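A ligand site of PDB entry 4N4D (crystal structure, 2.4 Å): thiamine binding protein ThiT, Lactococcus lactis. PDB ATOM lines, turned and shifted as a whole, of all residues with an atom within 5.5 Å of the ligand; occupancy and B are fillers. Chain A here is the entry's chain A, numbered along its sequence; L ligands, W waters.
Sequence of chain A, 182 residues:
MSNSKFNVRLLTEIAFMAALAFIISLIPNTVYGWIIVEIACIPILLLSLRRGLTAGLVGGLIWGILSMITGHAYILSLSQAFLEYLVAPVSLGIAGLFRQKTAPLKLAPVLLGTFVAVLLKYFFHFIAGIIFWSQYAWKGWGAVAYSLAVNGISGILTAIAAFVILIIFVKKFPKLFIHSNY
O1 of the ligand lies within hydrogen-bond range of OD1 of Asn 151 (2.6 Å). The side-chain carboxylate (OE1) of Glu 84 lies within hydrogen-bond range of a nitrogen (N1) of the ligand (2.7 Å). N1 of the ligand is in hydrogen-bond range of O of His 125, 3.0 Å away.
Water W1 bridges OH of Tyr 146 (2.6 Å) and N3 of the ligand (3.0 Å).
Residues that only touch the ligand: Trp 34, Tyr 122, Ala 128, Gly 129, Trp 133, Tyr 146, Val 150 and Ser 154. Hydrophobic or aromatic side chains that line the ligand: Trp 34, Tyr 122, His 125, Ala 128, Trp 133, Tyr 146 and Val 150. 11 residues have an atom within 4 Å of the ligand: Trp 34, Glu 84, Tyr 122, His 125, Ala 128, Gly 129, Trp 133, Tyr 146, Val 150, Asn 151 and Ser 154. The nearest printed residue that does not touch the ligand is Ile 36 (4.1 Å).
OG of Ser 147 sits at hydrogen-bond distance from ND2 of Asn 151 (2.9 Å). The side-chain carboxylate of Glu 84 is in hydrogen-bond range of a ring nitrogen (ND1) of His 125 (3.0 Å). OE2 of Glu 84 is in hydrogen-bond range of NE1 of Trp 133. The side-chain carboxylate (OE2) of Glu 84 is in hydrogen-bond range of the side-chain amide nitrogen (NE2) of Gln 80 (2.8 Å). A ring nitrogen (NE2) of His 125 lies within hydrogen-bond range of the side-chain amino group of Lys 121. The side-chain carboxylate (OE1) of Glu 38 is in hydrogen-bond range of the side-chain hydroxyl (OH) of Tyr 122. The backbone carbonyl oxygen (O) of Val 150 sits at hydrogen-bond distance from the side-chain hydroxyl (OG) of Ser 154 (2.9 Å). The side-chain hydroxyl (OG) of Ser 154 sits at hydrogen-bond distance from the backbone NH (N) of Ile 36 (2.8 Å).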
ATOM      1  N   TRP A  34      31.152   1.887 -26.125  1.00  0.00           N
ATOM      2  CA  TRP A  34      30.894   1.028 -24.966  1.00  0.00           C
ATOM      3  C   TRP A  34      31.879  -0.137 -24.883  1.00  0.00           C
ATOM      4  O   TRP A  34      31.669  -1.075 -24.162  1.00  0.00           O
ATOM      5  CB  TRP A  34      29.444   0.523 -24.999  1.00  0.00           C
ATOM      6  CG  TRP A  34      28.668   0.829 -23.746  1.00  0.00           C
ATOM      7  CD1 TRP A  34      27.543   1.594 -23.648  1.00  0.00           C
ATOM      8  CD2 TRP A  34      28.959   0.374 -22.408  1.00  0.00           C
ATOM      9  NE1 TRP A  34      27.119   1.639 -22.348  1.00  0.00           N
ATOM     10  CE2 TRP A  34      27.964   0.903 -21.569  1.00  0.00           C
ATOM     11  CE3 TRP A  34      29.967  -0.439 -21.840  1.00  0.00           C
ATOM     12  CZ2 TRP A  34      27.939   0.654 -20.189  1.00  0.00           C
ATOM     13  CZ3 TRP A  34      29.946  -0.684 -20.474  1.00  0.00           C
ATOM     14  CH2 TRP A  34      28.942  -0.139 -19.661  1.00  0.00           C
ATOM     15  N   ILE A  36      35.210  -1.721 -23.610  1.00  0.00           N
ATOM     16  CA  ILE A  36      35.944  -1.452 -22.387  1.00  0.00           C
ATOM     17  C   ILE A  36      36.937  -2.558 -22.054  1.00  0.00           C
ATOM     18  O   ILE A  36      36.826  -3.705 -22.509  1.00  0.00           O
ATOM     19  CB  ILE A  36      34.977  -1.233 -21.200  1.00  0.00           C
ATOM     20  CG1 ILE A  36      34.124  -2.480 -20.966  1.00  0.00           C
ATOM     21  CG2 ILE A  36      34.050  -0.076 -21.490  1.00  0.00           C
ATOM     22  CD1 ILE A  36      33.382  -2.463 -19.719  1.00  0.00           C
ATOM     23  N   GLU A  38      37.796  -4.420 -18.909  1.00  0.00           N
ATOM     24  CA  GLU A  38      37.219  -4.440 -17.577  1.00  0.00           C
ATOM     25  C   GLU A  38      38.185  -5.002 -16.476  1.00  0.00           C
ATOM     26  O   GLU A  38      37.866  -5.959 -15.777  1.00  0.00           O
ATOM     27  CB  GLU A  38      35.856  -5.102 -17.523  1.00  0.00           C
ATOM     28  CG  GLU A  38      35.097  -4.674 -16.255  1.00  0.00           C
ATOM     29  CD  GLU A  38      33.766  -5.321 -16.040  1.00  0.00           C
ATOM     30  OE1 GLU A  38      33.490  -6.370 -16.654  1.00  0.00           O
ATOM     31  OE2 GLU A  38      32.954  -4.767 -15.243  1.00  0.00           O
ATOM     32  N   TYR A  74      25.438   1.686 -14.908  1.00  0.00           N
ATOM     33  CA  TYR A  74      24.531   2.183 -15.939  1.00  0.00           C
ATOM     34  C   TYR A  74      23.227   1.402 -15.823  1.00  0.00           C
ATOM     35  O   TYR A  74      23.191   0.189 -16.086  1.00  0.00           O
ATOM     36  CB  TYR A  74      25.132   1.971 -17.316  1.00  0.00           C
ATOM     37  CG  TYR A  74      26.470   2.651 -17.521  1.00  0.00           C
ATOM     38  CD1 TYR A  74      26.527   3.990 -17.855  1.00  0.00           C
ATOM     39  CD2 TYR A  74      27.667   1.956 -17.404  1.00  0.00           C
ATOM     40  CE1 TYR A  74      27.738   4.622 -18.063  1.00  0.00           C
ATOM     41  CE2 TYR A  74      28.885   2.588 -17.595  1.00  0.00           C
ATOM     42  CZ  TYR A  74      28.909   3.930 -17.936  1.00  0.00           C
ATOM     43  OH  TYR A  74      30.101   4.585 -18.142  1.00  0.00           O
ATOM     44  N   GLN A  80      17.292  -5.151 -16.062  1.00  0.00           N
ATOM     45  CA  GLN A  80      18.571  -4.923 -16.765  1.00  0.00           C
ATOM     46  C   GLN A  80      19.737  -4.773 -15.775  1.00  0.00           C
ATOM     47  O   GLN A  80      20.778  -5.396 -15.949  1.00  0.00           O
ATOM     48  CB  GLN A  80      18.473  -3.696 -17.704  1.00  0.00           C
ATOM     49  CG  GLN A  80      19.827  -3.202 -18.227  1.00  0.00           C
ATOM     50  CD  GLN A  80      20.566  -2.235 -17.252  1.00  0.00           C
ATOM     51  OE1 GLN A  80      19.952  -1.541 -16.403  1.00  0.00           O
ATOM     52  NE2 GLN A  80      21.882  -2.205 -17.387  1.00  0.00           N
ATOM     53  N   GLU A  84      22.802  -7.158 -15.127  1.00  0.00           N
ATOM     54  CA  GLU A  84      24.147  -6.652 -15.393  1.00  0.00           C
ATOM     55  C   GLU A  84      25.022  -6.219 -14.215  1.00  0.00           C
ATOM     56  O   GLU A  84      26.238  -5.984 -14.382  1.00  0.00           O
ATOM     57  CB  GLU A  84      24.044  -5.479 -16.356  1.00  0.00           C
ATOM     58  CG  GLU A  84      23.653  -5.929 -17.735  1.00  0.00           C
ATOM     59  CD  GLU A  84      23.932  -4.869 -18.744  1.00  0.00           C
ATOM     60  OE1 GLU A  84      25.096  -4.846 -19.162  1.00  0.00           O
ATOM     61  OE2 GLU A  84      22.991  -4.088 -19.104  1.00  0.00           O
ATOM     62  N   TYR A  85      24.396  -6.048 -13.058  1.00  0.00           N
ATOM     63  CA  TYR A  85      25.106  -5.585 -11.884  1.00  0.00           C
ATOM     64  C   TYR A  85      24.868  -6.482 -10.640  1.00  0.00           C
ATOM     65  O   TYR A  85      25.295  -6.152  -9.542  1.00  0.00           O
ATOM     66  CB  TYR A  85      24.771  -4.105 -11.619  1.00  0.00           C
ATOM     67  CG  TYR A  85      25.429  -3.162 -12.624  1.00  0.00           C
ATOM     68  CD1 TYR A  85      26.751  -2.785 -12.459  1.00  0.00           C
ATOM     69  CD2 TYR A  85      24.744  -2.656 -13.732  1.00  0.00           C
ATOM     70  CE1 TYR A  85      27.372  -1.956 -13.354  1.00  0.00           C
ATOM     71  CE2 TYR A  85      25.381  -1.792 -14.652  1.00  0.00           C
ATOM     72  CZ  TYR A  85      26.688  -1.458 -14.457  1.00  0.00           C
ATOM     73  OH  TYR A  85      27.359  -0.592 -15.308  1.00  0.00           O
ATOM     74  N   LYS A 121      30.481 -13.887 -17.700  1.00  0.00           N
ATOM     75  CA  LYS A 121      30.044 -12.505 -17.485  1.00  0.00           C
ATOM     76  C   LYS A 121      29.653 -11.788 -18.786  1.00  0.00           C
ATOM     77  O   LYS A 121      28.603 -11.129 -18.866  1.00  0.00           O
ATOM     78  CB  LYS A 121      31.128 -11.681 -16.827  1.00  0.00           C
ATOM     79  CG  LYS A 121      30.587 -10.377 -16.266  1.00  0.00           C
ATOM     80  CD  LYS A 121      31.688  -9.518 -15.632  1.00  0.00           C
ATOM     81  CE  LYS A 121      31.116  -8.453 -14.694  1.00  0.00           C
ATOM     82  NZ  LYS A 121      31.245  -7.135 -15.296  1.00  0.00           N
ATOM     83  N   TYR A 122      30.502 -11.880 -19.791  1.00  0.00           N
ATOM     84  CA  TYR A 122      30.265 -11.121 -20.995  1.00  0.00           C
ATOM     85  C   TYR A 122      29.117 -11.773 -21.761  1.00  0.00           C
ATOM     86  O   TYR A 122      28.404 -11.121 -22.535  1.00  0.00           O
ATOM     87  CB  TYR A 122      31.562 -10.825 -21.765  1.00  0.00           C
ATOM     88  CG  TYR A 122      32.166  -9.618 -21.141  1.00  0.00           C
ATOM     89  CD1 TYR A 122      32.887  -9.701 -19.952  1.00  0.00           C
ATOM     90  CD2 TYR A 122      31.871  -8.354 -21.648  1.00  0.00           C
ATOM     91  CE1 TYR A 122      33.375  -8.545 -19.323  1.00  0.00           C
ATOM     92  CE2 TYR A 122      32.339  -7.198 -21.030  1.00  0.00           C
ATOM     93  CZ  TYR A 122      33.085  -7.287 -19.874  1.00  0.00           C
ATOM     94  OH  TYR A 122      33.509  -6.114 -19.277  1.00  0.00           O
ATOM     95  N   HIS A 125      26.256  -9.866 -20.392  1.00  0.00           N
ATOM     96  CA  HIS A 125      26.235  -8.535 -20.993  1.00  0.00           C
ATOM     97  C   HIS A 125      25.744  -8.536 -22.456  1.00  0.00           C
ATOM     98  O   HIS A 125      25.022  -7.654 -22.883  1.00  0.00           O
ATOM     99  CB  HIS A 125      27.630  -7.910 -20.893  1.00  0.00           C
ATOM    100  CG  HIS A 125      28.025  -7.571 -19.499  1.00  0.00           C
ATOM    101  ND1 HIS A 125      27.220  -6.832 -18.665  1.00  0.00           N
ATOM    102  CD2 HIS A 125      29.123  -7.914 -18.759  1.00  0.00           C
ATOM    103  CE1 HIS A 125      27.798  -6.711 -17.479  1.00  0.00           C
ATOM    104  NE2 HIS A 125      28.949  -7.358 -17.517  1.00  0.00           N
ATOM    105  N   PHE A 126      26.136  -9.559 -23.196  1.00  0.00           N
ATOM    106  CA  PHE A 126      25.694  -9.768 -24.564  1.00  0.00           C
ATOM    107  C   PHE A 126      24.166  -9.947 -24.635  1.00  0.00           C
ATOM    108  O   PHE A 126      23.506  -9.267 -25.435  1.00  0.00           O
ATOM    109  CB  PHE A 126      26.499 -10.942 -25.197  1.00  0.00           C
ATOM    110  CG  PHE A 126      25.828 -11.614 -26.383  1.00  0.00           C
ATOM    111  CD1 PHE A 126      25.832 -11.018 -27.655  1.00  0.00           C
ATOM    112  CD2 PHE A 126      25.263 -12.889 -26.245  1.00  0.00           C
ATOM    113  CE1 PHE A 126      25.257 -11.651 -28.735  1.00  0.00           C
ATOM    114  CE2 PHE A 126      24.694 -13.535 -27.327  1.00  0.00           C
ATOM    115  CZ  PHE A 126      24.679 -12.912 -28.574  1.00  0.00           C
ATOM    116  N   ALA A 128      22.129  -8.855 -22.401  1.00  0.00           N
ATOM    117  CA  ALA A 128      21.646  -7.525 -22.015  1.00  0.00           C
ATOM    118  C   ALA A 128      21.717  -6.520 -23.182  1.00  0.00           C
ATOM    119  O   ALA A 128      20.788  -5.754 -23.386  1.00  0.00           O
ATOM    120  CB  ALA A 128      22.401  -7.000 -20.814  1.00  0.00           C
ATOM    121  N   GLY A 129      22.819  -6.536 -23.916  1.00  0.00           N
ATOM    122  CA  GLY A 129      22.983  -5.706 -25.096  1.00  0.00           C
ATOM    123  C   GLY A 129      21.828  -5.902 -26.066  1.00  0.00           C
ATOM    124  O   GLY A 129      21.208  -4.926 -26.506  1.00  0.00           O
ATOM    125  N   TRP A 133      19.938  -2.537 -25.027  1.00  0.00           N
ATOM    126  CA  TRP A 133      20.901  -1.572 -25.548  1.00  0.00           C
ATOM    127  C   TRP A 133      20.866  -1.349 -27.060  1.00  0.00           C
ATOM    128  O   TRP A 133      21.715  -0.646 -27.581  1.00  0.00           O
ATOM    129  CB  TRP A 133      22.305  -1.981 -25.127  1.00  0.00           C
ATOM    130  CG  TRP A 133      22.508  -1.904 -23.660  1.00  0.00           C
ATOM    131  CD1 TRP A 133      22.450  -2.925 -22.757  1.00  0.00           C
ATOM    132  CD2 TRP A 133      22.780  -0.725 -22.906  1.00  0.00           C
ATOM    133  NE1 TRP A 133      22.694  -2.464 -21.489  1.00  0.00           N
ATOM    134  CE2 TRP A 133      22.893  -1.113 -21.550  1.00  0.00           C
ATOM    135  CE3 TRP A 133      22.943   0.630 -23.243  1.00  0.00           C
ATOM    136  CZ2 TRP A 133      23.168  -0.202 -20.525  1.00  0.00           C
ATOM    137  CZ3 TRP A 133      23.209   1.537 -22.221  1.00  0.00           C
ATOM    138  CH2 TRP A 133      23.329   1.116 -20.881  1.00  0.00           C
ATOM    139  N   TYR A 146      25.443  -6.016 -33.086  1.00  0.00           N
ATOM    140  CA  TYR A 146      25.986  -4.905 -32.300  1.00  0.00           C
ATOM    141  C   TYR A 146      26.407  -5.399 -30.907  1.00  0.00           C
ATOM    142  O   TYR A 146      27.456  -5.044 -30.418  1.00  0.00           O
ATOM    143  CB  TYR A 146      24.996  -3.738 -32.233  1.00  0.00           C
ATOM    144  CG  TYR A 146      25.382  -2.616 -31.283  1.00  0.00           C
ATOM    145  CD1 TYR A 146      26.574  -1.916 -31.438  1.00  0.00           C
ATOM    146  CD2 TYR A 146      24.539  -2.245 -30.244  1.00  0.00           C
ATOM    147  CE1 TYR A 146      26.918  -0.894 -30.555  1.00  0.00           C
ATOM    148  CE2 TYR A 146      24.875  -1.226 -29.363  1.00  0.00           C
ATOM    149  CZ  TYR A 146      26.063  -0.575 -29.518  1.00  0.00           C
ATOM    150  OH  TYR A 146      26.383   0.421 -28.633  1.00  0.00           O
ATOM    151  N   SER A 147      25.580  -6.221 -30.280  1.00  0.00           N
ATOM    152  CA  SER A 147      25.869  -6.668 -28.948  1.00  0.00           C
ATOM    153  C   SER A 147      27.066  -7.618 -28.977  1.00  0.00           C
ATOM    154  O   SER A 147      27.953  -7.464 -28.166  1.00  0.00           O
ATOM    155  CB  SER A 147      24.647  -7.290 -28.267  1.00  0.00           C
ATOM    156  OG  SER A 147      24.978  -7.651 -26.924  1.00  0.00           O
ATOM    157  N   VAL A 150      30.164  -5.315 -29.385  1.00  0.00           N
ATOM    158  CA  VAL A 150      30.534  -4.505 -28.225  1.00  0.00           C
ATOM    159  C   VAL A 150      31.038  -5.431 -27.100  1.00  0.00           C
ATOM    160  O   VAL A 150      32.090  -5.223 -26.486  1.00  0.00           O
ATOM    161  CB  VAL A 150      29.340  -3.726 -27.688  1.00  0.00           C
ATOM    162  CG1 VAL A 150      29.706  -3.020 -26.394  1.00  0.00           C
ATOM    163  CG2 VAL A 150      28.767  -2.712 -28.736  1.00  0.00           C
ATOM    164  N   ASN A 151      30.242  -6.461 -26.846  1.00  0.00           N
ATOM    165  CA  ASN A 151      30.441  -7.325 -25.717  1.00  0.00           C
ATOM    166  C   ASN A 151      31.477  -8.440 -25.954  1.00  0.00           C
ATOM    167  O   ASN A 151      32.296  -8.697 -25.070  1.00  0.00           O
ATOM    168  CB  ASN A 151      29.100  -7.832 -25.218  1.00  0.00           C
ATOM    169  CG  ASN A 151      28.250  -6.720 -24.649  1.00  0.00           C
ATOM    170  OD1 ASN A 151      28.625  -6.093 -23.636  1.00  0.00           O
ATOM    171  ND2 ASN A 151      27.080  -6.460 -25.278  1.00  0.00           N
ATOM    172  N   SER A 154      34.851  -6.400 -25.934  1.00  0.00           N
ATOM    173  CA  SER A 154      35.132  -6.035 -24.565  1.00  0.00           C
ATOM    174  C   SER A 154      35.512  -7.252 -23.683  1.00  0.00           C
ATOM    175  O   SER A 154      36.429  -7.191 -22.853  1.00  0.00           O
ATOM    176  CB  SER A 154      33.932  -5.316 -23.971  1.00  0.00           C
ATOM    177  OG  SER A 154      33.841  -4.004 -24.510  1.00  0.00           O
HETATM  178  C1  LIG L   1      25.586  -3.247 -26.474  1.00  0.00           C
HETATM  179  N1  LIG L   1      25.405  -4.909 -21.826  1.00  0.00           N
HETATM  180  O1  LIG L   1      30.413  -4.373 -22.720  1.00  0.00           O
HETATM  181  C2  LIG L   1      30.468  -4.816 -21.287  1.00  0.00           C
HETATM  182  C3  LIG L   1      27.515  -2.953 -18.743  1.00  0.00           C
HETATM  183  C4  LIG L   1      29.435  -4.160 -20.375  1.00  0.00           C
HETATM  184  C5  LIG L   1      28.310  -3.538 -20.946  1.00  0.00           C
HETATM  185  C6  LIG L   1      27.326  -2.928 -20.096  1.00  0.00           C
HETATM  186  C7  LIG L   1      26.066  -2.231 -20.721  1.00  0.00           C
HETATM  187  C8  LIG L   1      25.627  -3.794 -22.720  1.00  0.00           C
HETATM  188  N2  LIG L   1      25.521  -3.993 -24.103  1.00  0.00           N
HETATM  189  C9  LIG L   1      25.709  -3.002 -24.956  1.00  0.00           C
HETATM  190  N3  LIG L   1      26.023  -1.786 -24.519  1.00  0.00           N
HETATM  191  C10 LIG L   1      26.138  -1.489 -23.175  1.00  0.00           C
HETATM  192  C11 LIG L   1      25.936  -2.507 -22.213  1.00  0.00           C
HETATM  193  C12 LIG L   1      29.612  -4.192 -19.011  1.00  0.00           C
HETATM  194  C13 LIG L   1      28.635  -3.571 -18.164  1.00  0.00           C
HETATM  195  O   HOH W   1      25.479   0.583 -26.218  1.00  0.00           O
HETATM  196  O   HOH W   2      30.113  -3.392 -15.570  1.00  0.00           O
